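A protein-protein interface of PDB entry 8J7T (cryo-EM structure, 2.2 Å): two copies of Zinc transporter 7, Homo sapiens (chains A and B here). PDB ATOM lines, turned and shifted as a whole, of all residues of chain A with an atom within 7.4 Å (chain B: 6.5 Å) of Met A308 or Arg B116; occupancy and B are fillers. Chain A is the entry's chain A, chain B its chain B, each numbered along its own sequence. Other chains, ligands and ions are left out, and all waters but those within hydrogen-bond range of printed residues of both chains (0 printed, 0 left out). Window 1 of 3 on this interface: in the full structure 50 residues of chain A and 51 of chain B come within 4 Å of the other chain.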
ATOM      1  N   ARG A 116      -1.374 -13.470  10.035  1.00  0.00           N
ATOM      2  CA  ARG A 116      -1.338 -12.334   9.120  1.00  0.00           C
ATOM      3  C   ARG A 116       0.081 -11.997   8.692  1.00  0.00           C
ATOM      4  O   ARG A 116       0.276 -11.380   7.640  1.00  0.00           O
ATOM      5  CB  ARG A 116      -1.994 -11.113   9.766  1.00  0.00           C
ATOM      6  CG  ARG A 116      -3.469 -10.974   9.466  1.00  0.00           C
ATOM      7  CD  ARG A 116      -3.692 -10.436   8.073  1.00  0.00           C
ATOM      8  NE  ARG A 116      -5.104 -10.449   7.717  1.00  0.00           N
ATOM      9  CZ  ARG A 116      -5.905  -9.396   7.775  1.00  0.00           C
ATOM     10  NH1 ARG A 116      -5.464  -8.214   8.163  1.00  0.00           N
ATOM     11  NH2 ARG A 116      -7.179  -9.533   7.432  1.00  0.00           N
ATOM     12  N   GLU A 302      -3.654  -9.450  -4.335  1.00  0.00           N
ATOM     13  CA  GLU A 302      -4.177 -10.384  -3.347  1.00  0.00           C
ATOM     14  C   GLU A 302      -3.877  -9.907  -1.927  1.00  0.00           C
ATOM     15  O   GLU A 302      -4.766  -9.891  -1.063  1.00  0.00           O
ATOM     16  CB  GLU A 302      -3.588 -11.764  -3.628  1.00  0.00           C
ATOM     17  CG  GLU A 302      -4.558 -12.915  -3.476  1.00  0.00           C
ATOM     18  CD  GLU A 302      -4.937 -13.178  -2.050  1.00  0.00           C
ATOM     19  OE1 GLU A 302      -4.020 -13.191  -1.213  1.00  0.00           O
ATOM     20  OE2 GLU A 302      -6.137 -13.404  -1.778  1.00  0.00           O
ATOM     21  N   SER A 303      -2.643  -9.451  -1.686  1.00  0.00           N
ATOM     22  CA  SER A 303      -2.259  -8.980  -0.358  1.00  0.00           C
ATOM     23  C   SER A 303      -3.035  -7.734   0.044  1.00  0.00           C
ATOM     24  O   SER A 303      -3.472  -7.615   1.195  1.00  0.00           O
ATOM     25  CB  SER A 303      -0.758  -8.701  -0.307  1.00  0.00           C
ATOM     26  OG  SER A 303      -0.001  -9.845  -0.639  1.00  0.00           O
ATOM     27  N   VAL A 304      -3.199  -6.783  -0.878  1.00  0.00           N
ATOM     28  CA  VAL A 304      -3.931  -5.562  -0.561  1.00  0.00           C
ATOM     29  C   VAL A 304      -5.395  -5.874  -0.294  1.00  0.00           C
ATOM     30  O   VAL A 304      -5.997  -5.323   0.634  1.00  0.00           O
ATOM     31  CB  VAL A 304      -3.755  -4.522  -1.686  1.00  0.00           C
ATOM     32  CG1 VAL A 304      -4.762  -3.407  -1.547  1.00  0.00           C
ATOM     33  CG2 VAL A 304      -2.352  -3.951  -1.647  1.00  0.00           C
ATOM     34  N   GLY A 305      -5.993  -6.770  -1.084  1.00  0.00           N
ATOM     35  CA  GLY A 305      -7.356  -7.177  -0.801  1.00  0.00           C
ATOM     36  C   GLY A 305      -7.507  -7.776   0.582  1.00  0.00           C
ATOM     37  O   GLY A 305      -8.468  -7.484   1.294  1.00  0.00           O
ATOM     38  N   ILE A 306      -6.553  -8.613   0.990  1.00  0.00           N
ATOM     39  CA  ILE A 306      -6.619  -9.163   2.340  1.00  0.00           C
ATOM     40  C   ILE A 306      -6.467  -8.062   3.385  1.00  0.00           C
ATOM     41  O   ILE A 306      -7.178  -8.044   4.394  1.00  0.00           O
ATOM     42  CB  ILE A 306      -5.569 -10.271   2.528  1.00  0.00           C
ATOM     43  CG1 ILE A 306      -5.920 -11.480   1.669  1.00  0.00           C
ATOM     44  CG2 ILE A 306      -5.464 -10.661   3.991  1.00  0.00           C
ATOM     45  CD1 ILE A 306      -4.832 -12.489   1.613  1.00  0.00           C
ATOM     46  N   LEU A 307      -5.544  -7.127   3.163  1.00  0.00           N
ATOM     47  CA  LEU A 307      -5.238  -6.125   4.177  1.00  0.00           C
ATOM     48  C   LEU A 307      -6.268  -5.005   4.248  1.00  0.00           C
ATOM     49  O   LEU A 307      -6.308  -4.292   5.253  1.00  0.00           O
ATOM     50  CB  LEU A 307      -3.846  -5.543   3.931  1.00  0.00           C
ATOM     51  CG  LEU A 307      -2.694  -6.505   4.222  1.00  0.00           C
ATOM     52  CD1 LEU A 307      -1.365  -5.841   3.969  1.00  0.00           C
ATOM     53  CD2 LEU A 307      -2.770  -7.030   5.655  1.00  0.00           C
ATOM     54  N   MET A 308      -7.105  -4.838   3.227  1.00  0.00           N
ATOM     55  CA  MET A 308      -8.189  -3.868   3.282  1.00  0.00           C
ATOM     56  C   MET A 308      -9.479  -4.448   3.829  1.00  0.00           C
ATOM     57  O   MET A 308     -10.519  -3.797   3.722  1.00  0.00           O
ATOM     58  CB  MET A 308      -8.458  -3.252   1.906  1.00  0.00           C
ATOM     59  CG  MET A 308      -7.279  -2.558   1.270  1.00  0.00           C
ATOM     60  SD  MET A 308      -7.260  -0.799   1.668  1.00  0.00           S
ATOM     61  CE  MET A 308      -8.917  -0.294   1.233  1.00  0.00           C
ATOM     62  N   GLN A 309      -9.432  -5.648   4.414  1.00  0.00           N
ATOM     63  CA  GLN A 309     -10.617  -6.345   4.911  1.00  0.00           C
ATOM     64  C   GLN A 309     -11.661  -6.515   3.814  1.00  0.00           C
ATOM     65  O   GLN A 309     -12.857  -6.357   4.048  1.00  0.00           O
ATOM     66  CB  GLN A 309     -11.219  -5.635   6.128  1.00  0.00           C
ATOM     67  CG  GLN A 309     -10.257  -5.445   7.289  1.00  0.00           C
ATOM     68  CD  GLN A 309      -9.785  -6.760   7.891  1.00  0.00           C
ATOM     69  OE1 GLN A 309      -8.657  -7.180   7.675  1.00  0.00           O
ATOM     70  NE2 GLN A 309     -10.647  -7.399   8.663  1.00  0.00           N
ATOM     71  N   ARG A 310     -11.203  -6.822   2.607  1.00  0.00           N
ATOM     72  CA  ARG A 310     -12.096  -7.063   1.488  1.00  0.00           C
ATOM     73  C   ARG A 310     -12.764  -8.429   1.623  1.00  0.00           C
ATOM     74  O   ARG A 310     -12.256  -9.331   2.290  1.00  0.00           O
ATOM     75  CB  ARG A 310     -11.320  -6.975   0.174  1.00  0.00           C
ATOM     76  CG  ARG A 310     -12.152  -6.972  -1.083  1.00  0.00           C
ATOM     77  CD  ARG A 310     -11.304  -7.330  -2.278  1.00  0.00           C
ATOM     78  NE  ARG A 310     -12.049  -7.324  -3.531  1.00  0.00           N
ATOM     79  CZ  ARG A 310     -12.967  -8.219  -3.868  1.00  0.00           C
ATOM     80  NH1 ARG A 310     -13.308  -9.202  -3.052  1.00  0.00           N
ATOM     81  NH2 ARG A 310     -13.554  -8.128  -5.054  1.00  0.00           N
ATOM     82  N   THR A 311     -13.920  -8.564   0.996  1.00  0.00           N
ATOM     83  CA  THR A 311     -14.586  -9.853   0.922  1.00  0.00           C
ATOM     84  C   THR A 311     -13.676 -10.842   0.203  1.00  0.00           C
ATOM     85  O   THR A 311     -13.118 -10.505  -0.847  1.00  0.00           O
ATOM     86  CB  THR A 311     -15.913  -9.719   0.176  1.00  0.00           C
ATOM     87  OG1 THR A 311     -16.705  -8.692   0.779  1.00  0.00           O
ATOM     88  CG2 THR A 311     -16.678 -11.018   0.207  1.00  0.00           C
ATOM     89  N   TRP A 341     -14.222 -11.480   5.642  1.00  0.00           N
ATOM     90  CA  TRP A 341     -12.874 -11.058   5.309  1.00  0.00           C
ATOM     91  C   TRP A 341     -11.916 -12.231   5.430  1.00  0.00           C
ATOM     92  O   TRP A 341     -12.236 -13.280   5.988  1.00  0.00           O
ATOM     93  CB  TRP A 341     -12.411  -9.881   6.179  1.00  0.00           C
ATOM     94  CG  TRP A 341     -12.652 -10.013   7.649  1.00  0.00           C
ATOM     95  CD1 TRP A 341     -13.807  -9.753   8.316  1.00  0.00           C
ATOM     96  CD2 TRP A 341     -11.698 -10.411   8.639  1.00  0.00           C
ATOM     97  NE1 TRP A 341     -13.637  -9.965   9.658  1.00  0.00           N
ATOM     98  CE2 TRP A 341     -12.350 -10.369   9.885  1.00  0.00           C
ATOM     99  CE3 TRP A 341     -10.355 -10.793   8.592  1.00  0.00           C
ATOM    100  CZ2 TRP A 341     -11.711 -10.704  11.074  1.00  0.00           C
ATOM    101  CZ3 TRP A 341      -9.721 -11.124   9.770  1.00  0.00           C
ATOM    102  CH2 TRP A 341     -10.400 -11.082  10.997  1.00  0.00           C
ATOM    103  N   ILE B 101      -9.568   7.790  -1.183  1.00  0.00           N
ATOM    104  CA  ILE B 101     -10.273   6.515  -1.251  1.00  0.00           C
ATOM    105  C   ILE B 101     -10.933   6.169   0.080  1.00  0.00           C
ATOM    106  O   ILE B 101     -11.969   5.495   0.106  1.00  0.00           O
ATOM    107  CB  ILE B 101      -9.295   5.425  -1.725  1.00  0.00           C
ATOM    108  CG1 ILE B 101      -8.885   5.690  -3.172  1.00  0.00           C
ATOM    109  CG2 ILE B 101      -9.893   4.043  -1.603  1.00  0.00           C
ATOM    110  CD1 ILE B 101      -7.664   4.915  -3.611  1.00  0.00           C
ATOM    111  N   SER B 102     -10.369   6.634   1.197  1.00  0.00           N
ATOM    112  CA  SER B 102     -10.907   6.285   2.506  1.00  0.00           C
ATOM    113  C   SER B 102     -12.349   6.730   2.682  1.00  0.00           C
ATOM    114  O   SER B 102     -13.092   6.093   3.435  1.00  0.00           O
ATOM    115  CB  SER B 102     -10.040   6.901   3.600  1.00  0.00           C
ATOM    116  OG  SER B 102      -8.964   6.045   3.937  1.00  0.00           O
ATOM    117  N   PHE B 110     -16.059  -4.532  -0.641  1.00  0.00           N
ATOM    118  CA  PHE B 110     -15.416  -3.869   0.487  1.00  0.00           C
ATOM    119  C   PHE B 110     -16.502  -3.507   1.493  1.00  0.00           C
ATOM    120  O   PHE B 110     -16.973  -2.371   1.551  1.00  0.00           O
ATOM    121  CB  PHE B 110     -14.631  -2.654   0.007  1.00  0.00           C
ATOM    122  CG  PHE B 110     -13.441  -3.011  -0.823  1.00  0.00           C
ATOM    123  CD1 PHE B 110     -13.580  -3.284  -2.172  1.00  0.00           C
ATOM    124  CD2 PHE B 110     -12.188  -3.109  -0.252  1.00  0.00           C
ATOM    125  CE1 PHE B 110     -12.490  -3.630  -2.935  1.00  0.00           C
ATOM    126  CE2 PHE B 110     -11.095  -3.451  -1.015  1.00  0.00           C
ATOM    127  CZ  PHE B 110     -11.246  -3.712  -2.357  1.00  0.00           C
ATOM    128  N   TYR B 112     -16.445  -3.205   4.711  1.00  0.00           N
ATOM    129  CA  TYR B 112     -16.038  -2.237   5.715  1.00  0.00           C
ATOM    130  C   TYR B 112     -15.715  -0.879   5.119  1.00  0.00           C
ATOM    131  O   TYR B 112     -15.306   0.024   5.852  1.00  0.00           O
ATOM    132  CB  TYR B 112     -14.821  -2.756   6.479  1.00  0.00           C
ATOM    133  CG  TYR B 112     -15.125  -3.874   7.436  1.00  0.00           C
ATOM    134  CD1 TYR B 112     -15.757  -3.626   8.643  1.00  0.00           C
ATOM    135  CD2 TYR B 112     -14.777  -5.180   7.137  1.00  0.00           C
ATOM    136  CE1 TYR B 112     -16.028  -4.645   9.525  1.00  0.00           C
ATOM    137  CE2 TYR B 112     -15.048  -6.204   8.009  1.00  0.00           C
ATOM    138  CZ  TYR B 112     -15.672  -5.930   9.202  1.00  0.00           C
ATOM    139  OH  TYR B 112     -15.943  -6.951  10.073  1.00  0.00           O
ATOM    140  N   GLY B 113     -15.890  -0.711   3.815  1.00  0.00           N
ATOM    141  CA  GLY B 113     -15.455   0.491   3.146  1.00  0.00           C
ATOM    142  C   GLY B 113     -13.991   0.404   2.779  1.00  0.00           C
ATOM    143  O   GLY B 113     -13.437  -0.692   2.671  1.00  0.00           O
ATOM    144  N   TYR B 114     -13.351   1.550   2.595  1.00  0.00           N
ATOM    145  CA  TYR B 114     -11.961   1.611   2.166  1.00  0.00           C
ATOM    146  C   TYR B 114     -11.100   2.324   3.195  1.00  0.00           C
ATOM    147  O   TYR B 114     -10.093   2.936   2.850  1.00  0.00           O
ATOM    148  CB  TYR B 114     -11.847   2.307   0.812  1.00  0.00           C
ATOM    149  CG  TYR B 114     -12.554   1.607  -0.314  1.00  0.00           C
ATOM    150  CD1 TYR B 114     -13.897   1.846  -0.570  1.00  0.00           C
ATOM    151  CD2 TYR B 114     -11.881   0.711  -1.126  1.00  0.00           C
ATOM    152  CE1 TYR B 114     -14.549   1.209  -1.602  1.00  0.00           C
ATOM    153  CE2 TYR B 114     -12.524   0.068  -2.157  1.00  0.00           C
ATOM    154  CZ  TYR B 114     -13.857   0.322  -2.391  1.00  0.00           C
ATOM    155  OH  TYR B 114     -14.494  -0.317  -3.420  1.00  0.00           O
ATOM    156  N   VAL B 115     -11.502   2.267   4.464  1.00  0.00           N
ATOM    157  CA  VAL B 115     -10.812   3.026   5.500  1.00  0.00           C
ATOM    158  C   VAL B 115      -9.417   2.463   5.743  1.00  0.00           C
ATOM    159  O   VAL B 115      -8.486   3.204   6.086  1.00  0.00           O
ATOM    160  CB  VAL B 115     -11.660   3.053   6.781  1.00  0.00           C
ATOM    161  CG1 VAL B 115     -12.891   3.910   6.566  1.00  0.00           C
ATOM    162  CG2 VAL B 115     -12.054   1.645   7.196  1.00  0.00           C
ATOM    163  N   ARG B 116      -9.242   1.155   5.535  1.00  0.00           N
ATOM    164  CA  ARG B 116      -7.945   0.523   5.759  1.00  0.00           C
ATOM    165  C   ARG B 116      -6.862   1.127   4.880  1.00  0.00           C
ATOM    166  O   ARG B 116      -5.677   1.033   5.213  1.00  0.00           O
ATOM    167  CB  ARG B 116      -8.039  -0.984   5.509  1.00  0.00           C
ATOM    168  CG  ARG B 116      -8.355  -1.795   6.746  1.00  0.00           C
ATOM    169  CD  ARG B 116      -7.134  -1.953   7.618  1.00  0.00           C
ATOM    170  NE  ARG B 116      -7.462  -2.593   8.884  1.00  0.00           N
ATOM    171  CZ  ARG B 116      -7.274  -3.877   9.149  1.00  0.00           C
ATOM    172  NH1 ARG B 116      -6.746  -4.696   8.258  1.00  0.00           N
ATOM    173  NH2 ARG B 116      -7.621  -4.348  10.340  1.00  0.00           N
ATOM    174  N   ALA B 117      -7.252   1.760   3.769  1.00  0.00           N
ATOM    175  CA  ALA B 117      -6.287   2.450   2.924  1.00  0.00           C
ATOM    176  C   ALA B 117      -5.422   3.390   3.744  1.00  0.00           C
ATOM    177  O   ALA B 117      -4.195   3.411   3.587  1.00  0.00           O
ATOM    178  CB  ALA B 117      -7.011   3.222   1.823  1.00  0.00           C
ATOM    179  N   GLU B 118      -6.039   4.127   4.672  1.00  0.00           N
ATOM    180  CA  GLU B 118      -5.277   5.018   5.535  1.00  0.00           C
ATOM    181  C   GLU B 118      -4.137   4.269   6.205  1.00  0.00           C
ATOM    182  O   GLU B 118      -2.963   4.625   6.041  1.00  0.00           O
ATOM    183  CB  GLU B 118      -6.206   5.643   6.578  1.00  0.00           C
ATOM    184  CG  GLU B 118      -5.502   6.389   7.692  1.00  0.00           C
ATOM    185  CD  GLU B 118      -5.944   5.926   9.065  1.00  0.00           C
ATOM    186  OE1 GLU B 118      -6.689   4.929   9.144  1.00  0.00           O
ATOM    187  OE2 GLU B 118      -5.543   6.551  10.068  1.00  0.00           O
ATOM    188  N   VAL B 119      -4.462   3.157   6.870  1.00  0.00           N
ATOM    189  CA  VAL B 119      -3.433   2.357   7.523  1.00  0.00           C
ATOM    190  C   VAL B 119      -2.377   1.948   6.510  1.00  0.00           C
ATOM    191  O   VAL B 119      -1.175   2.160   6.719  1.00  0.00           O
ATOM    192  CB  VAL B 119      -4.060   1.131   8.213  1.00  0.00           C
ATOM    193  CG1 VAL B 119      -2.980   0.245   8.812  1.00  0.00           C
ATOM    194  CG2 VAL B 119      -5.051   1.564   9.270  1.00  0.00           C
ATOM    195  N   LEU B 120      -2.818   1.430   5.359  1.00  0.00           N
ATOM    196  CA  LEU B 120      -1.865   0.972   4.359  1.00  0.00           C
ATOM    197  C   LEU B 120      -0.930   2.096   3.954  1.00  0.00           C
ATOM    198  O   LEU B 120       0.289   1.895   3.875  1.00  0.00           O
ATOM    199  CB  LEU B 120      -2.595   0.410   3.142  1.00  0.00           C
ATOM    200  CG  LEU B 120      -3.102  -1.025   3.254  1.00  0.00           C
ATOM    201  CD1 LEU B 120      -3.723  -1.461   1.947  1.00  0.00           C
ATOM    202  CD2 LEU B 120      -1.976  -1.963   3.649  1.00  0.00           C
ATOM    203  N   ALA B 121      -1.473   3.303   3.761  1.00  0.00           N
ATOM    204  CA  ALA B 121      -0.629   4.423   3.373  1.00  0.00           C
ATOM    205  C   ALA B 121       0.507   4.588   4.364  1.00  0.00           C
ATOM    206  O   ALA B 121       1.684   4.591   3.982  1.00  0.00           O
ATOM    207  CB  ALA B 121      -1.453   5.706   3.279  1.00  0.00           C
ATOM    208  N   PRO B 243     -10.722   8.777   8.495  1.00  0.00           N
ATOM    209  CA  PRO B 243      -9.406   8.310   8.947  1.00  0.00           C
ATOM    210  C   PRO B 243      -8.269   9.062   8.264  1.00  0.00           C
ATOM    211  O   PRO B 243      -8.137   8.982   7.045  1.00  0.00           O
ATOM    212  CB  PRO B 243      -9.397   6.826   8.547  1.00  0.00           C
ATOM    213  CG  PRO B 243     -10.530   6.661   7.582  1.00  0.00           C
ATOM    214  CD  PRO B 243     -11.548   7.673   7.980  1.00  0.00           C
ATOM    215  N   ILE B 306      -2.122  -2.943  13.583  1.00  0.00           N
ATOM    216  CA  ILE B 306      -3.439  -2.917  12.954  1.00  0.00           C
ATOM    217  C   ILE B 306      -3.557  -4.009  11.895  1.00  0.00           C
ATOM    218  O   ILE B 306      -4.586  -4.685  11.795  1.00  0.00           O
ATOM    219  CB  ILE B 306      -3.735  -1.527  12.368  1.00  0.00           C
ATOM    220  CG1 ILE B 306      -3.892  -0.506  13.489  1.00  0.00           C
ATOM    221  CG2 ILE B 306      -4.978  -1.570  11.499  1.00  0.00           C
ATOM    222  CD1 ILE B 306      -3.939   0.894  12.998  1.00  0.00           C
ATOM    223  N   LEU B 307      -2.513  -4.204  11.091  1.00  0.00           N
ATOM    224  CA  LEU B 307      -2.599  -5.126   9.966  1.00  0.00           C
ATOM    225  C   LEU B 307      -2.478  -6.588  10.375  1.00  0.00           C
ATOM    226  O   LEU B 307      -2.855  -7.461   9.589  1.00  0.00           O
ATOM    227  CB  LEU B 307      -1.530  -4.782   8.928  1.00  0.00           C
ATOM    228  CG  LEU B 307      -1.782  -3.482   8.163  1.00  0.00           C
ATOM    229  CD1 LEU B 307      -0.690  -3.235   7.154  1.00  0.00           C
ATOM    230  CD2 LEU B 307      -3.150  -3.505   7.484  1.00  0.00           C
ATOM    231  N   MET B 308      -1.982  -6.880  11.575  1.00  0.00           N
ATOM    232  CA  MET B 308      -1.954  -8.248  12.074  1.00  0.00           C
ATOM    233  C   MET B 308      -3.201  -8.624  12.851  1.00  0.00           C
ATOM    234  O   MET B 308      -3.204  -9.667  13.506  1.00  0.00           O
ATOM    235  CB  MET B 308      -0.722  -8.497  12.949  1.00  0.00           C
ATOM    236  CG  MET B 308       0.605  -8.246  12.277  1.00  0.00           C
ATOM    237  SD  MET B 308       1.260  -9.753  11.534  1.00  0.00           S
ATOM    238  CE  MET B 308       1.164 -10.916  12.886  1.00  0.00           C
ATOM    239  N   GLN B 309      -4.253  -7.804  12.788  1.00  0.00           N
ATOM    240  CA  GLN B 309      -5.483  -8.016  13.550  1.00  0.00           C
ATOM    241  C   GLN B 309      -5.197  -8.127  15.043  1.00  0.00           C
ATOM    242  O   GLN B 309      -5.780  -8.956  15.739  1.00  0.00           O
ATOM    243  CB  GLN B 309      -6.249  -9.246  13.051  1.00  0.00           C
ATOM    244  CG  GLN B 309      -6.606  -9.211  11.574  1.00  0.00           C
ATOM    245  CD  GLN B 309      -7.557  -8.079  11.218  1.00  0.00           C
ATOM    246  OE1 GLN B 309      -7.155  -7.083  10.633  1.00  0.00           O
ATOM    247  NE2 GLN B 309      -8.824  -8.243  11.556  1.00  0.00           N
ATOM    248  N   TRP B 341     -10.257  -6.035  17.182  1.00  0.00           N
ATOM    249  CA  TRP B 341      -9.228  -5.562  16.274  1.00  0.00           C
ATOM    250  C   TRP B 341      -9.546  -4.149  15.815  1.00  0.00           C
ATOM    251  O   TRP B 341     -10.652  -3.637  15.997  1.00  0.00           O
ATOM    252  CB  TRP B 341      -9.049  -6.501  15.072  1.00  0.00           C
ATOM    253  CG  TRP B 341     -10.302  -6.935  14.383  1.00  0.00           C
ATOM    254  CD1 TRP B 341     -11.133  -7.945  14.755  1.00  0.00           C
ATOM    255  CD2 TRP B 341     -10.850  -6.387  13.179  1.00  0.00           C
ATOM    256  NE1 TRP B 341     -12.165  -8.062  13.863  1.00  0.00           N
ATOM    257  CE2 TRP B 341     -12.016  -7.118  12.883  1.00  0.00           C
ATOM    258  CE3 TRP B 341     -10.464  -5.356  12.321  1.00  0.00           C
ATOM    259  CZ2 TRP B 341     -12.807  -6.844  11.773  1.00  0.00           C
ATOM    260  CZ3 TRP B 341     -11.247  -5.085  11.220  1.00  0.00           C
ATOM    261  CH2 TRP B 341     -12.409  -5.824  10.956  1.00  0.00           C
ATOM    262  N   THR B 342      -8.545  -3.517  15.224  1.00  0.00           N
ATOM    263  CA  THR B 342      -8.640  -2.149  14.744  1.00  0.00           C
ATOM    264  C   THR B 342      -8.955  -2.163  13.254  1.00  0.00           C
ATOM    265  O   THR B 342      -8.190  -2.716  12.462  1.00  0.00           O
ATOM    266  CB  THR B 342      -7.339  -1.394  15.014  1.00  0.00           C
ATOM    267  OG1 THR B 342      -6.985  -1.527  16.394  1.00  0.00           O
ATOM    268  CG2 THR B 342      -7.479   0.062  14.661  1.00  0.00           C
ATOM    269  N   LEU B 343     -10.083  -1.563  12.886  1.00  0.00           N
ATOM    270  CA  LEU B 343     -10.395  -1.362  11.477  1.00  0.00           C
ATOM    271  C   LEU B 343      -9.612  -0.182  10.919  1.00  0.00           C
ATOM    272  O   LEU B 343      -8.927  -0.304   9.902  1.00  0.00           O
ATOM    273  CB  LEU B 343     -11.898  -1.150  11.297  1.00  0.00           C
ATOM    274  CG  LEU B 343     -12.406  -0.885   9.881  1.00  0.00           C
ATOM    275  CD1 LEU B 343     -11.951  -1.959   8.899  1.00  0.00           C
ATOM    276  CD2 LEU B 343     -13.915  -0.741   9.866  1.00  0.00           C
ATOM    277  N   CYS B 344      -9.708   0.963  11.582  1.00  0.00           N
ATOM    278  CA  CYS B 344      -8.876   2.121  11.305  1.00  0.00           C
ATOM    279  C   CYS B 344      -8.743   2.890  12.611  1.00  0.00           C
ATOM    280  O   CYS B 344      -9.157   2.413  13.670  1.00  0.00           O
ATOM    281  CB  CYS B 344      -9.463   2.985  10.183  1.00  0.00           C
ATOM    282  SG  CYS B 344     -11.222   3.341  10.347  1.00  0.00           S
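Arg A116 touches Gln B309, and with the chains exchanged Gln A309 touches Arg B116. Leu A307 touches its own counterpart, Leu B307. Gln B309 touches its own counterpart, Gln A309. Gln A309 touches Trp B341, and with the chains exchanged Trp A341 touches Gln B309. 6 positions are printed for both chains. Of the 20 pairs that touch across the chains among the printed residues, 12 have their exchanged pair printed and touching as well.
The backbone carbonyl oxygen (O) of Ile A306 lies within hydrogen-bond range of the guanidinium group (NH2) of Arg A116, at 3.4 Å. NH2 of Arg A116 sits at hydrogen-bond distance from OE1 of Gln A309. The backbone carbonyl oxygen (O) of Gly A305 sits at hydrogen-bond distance from the backbone NH (N) of Arg A310. The side-chain hydroxyl (OG) of Ser B102 lies close to the backbone carbonyl oxygen (O) of Tyr B114, 3.5 Å away. O of Ile B306 is in hydrogen-bond range of NH2 of Arg B116 (3.4 Å). NE of Arg B116 sits at hydrogen-bond distance from O of Leu B343 (2.9 Å).
Met A308 touches just these residues of chain B: Phe B110 (3.9 Å), Tyr B114 (3.7 Å), Arg B116 (3.6 Å), Ala B117 (3.3 Å) and Leu B120 (3.6 Å). Ile B101 touches none of the printed residues of chain A. Of the printed residues of chain A, Phe B110 touches Met A308 and Arg A310. Val B119 touches none of the printed residues of chain A. Printed residues of chain A within 4 Å of Leu B120: Leu A307 and Met A308. Of the printed residues of chain A, Met B308 touches Arg A116. Printed residues of chain A within 4 Å of Trp B341: Gln A309 (3.3 Å) and Trp A341 (3.9 Å). The nearest printed residue of chain A that does not touch Leu B307 is Met A308 (6.0 Å).
The guanidinium group (NH1) of Arg A116 is in hydrogen-bond range of the backbone carbonyl oxygen (O) of Leu B307, at 3.1 Å. The guanidinium group (NH1) of Arg A116 sits at hydrogen-bond distance from the side-chain amide oxygen (OE1) of Gln B309, 3.2 Å away. The backbone carbonyl oxygen (O) of Leu A307 is in hydrogen-bond range of the guanidinium group (NH1) of Arg B116 (3.1 Å). The backbone NH of Ala B117 sits at hydrogen-bond distance from the side-chain sulfur of Met A308 (3.3 Å). The guanidinium group (NH1) of Arg B116 is in hydrogen-bond range of the side-chain amide oxygen (OE1) of Gln A309, at 3.2 Å. The side-chain amide oxygen (OE1) of Gln A309 sits close to the side-chain amide oxygen (OE1) of Gln B309, at 3.3 Å.
Among the printed residues, pairs that only touch across the chains: Gln A309 with Trp B341, Trp A341 with Gln B309, Met A308 with Leu B120, Arg A310 with Phe B110, Met A308 with Arg B116, Arg A116 with Met B308, Met A308 with Tyr B114, Gln A309 with Tyr B112, Arg A116 with Arg B116, Trp A341 with Tyr B112, Trp A341 with Trp B341, Leu A307 with Leu B120, Met A308 with Phe B110 and Leu A307 with Leu B307.
Hydrophobic or aromatic side chains of chain B that line the printed part of chain A: Phe B110, Tyr B112, Tyr B114, Leu B120, Leu B307, Met B308 and Trp B341. Hydrophobic or aromatic side chains of chain A that line the printed part of chain B: Leu A307, Met A308 and Trp A341. Among the printed residues, 20 pairs touch across the chains. Among the printed residues, no Asp or Glu carboxylate lies within 4 Å of a Lys or Arg side-chain nitrogen of the other chain.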
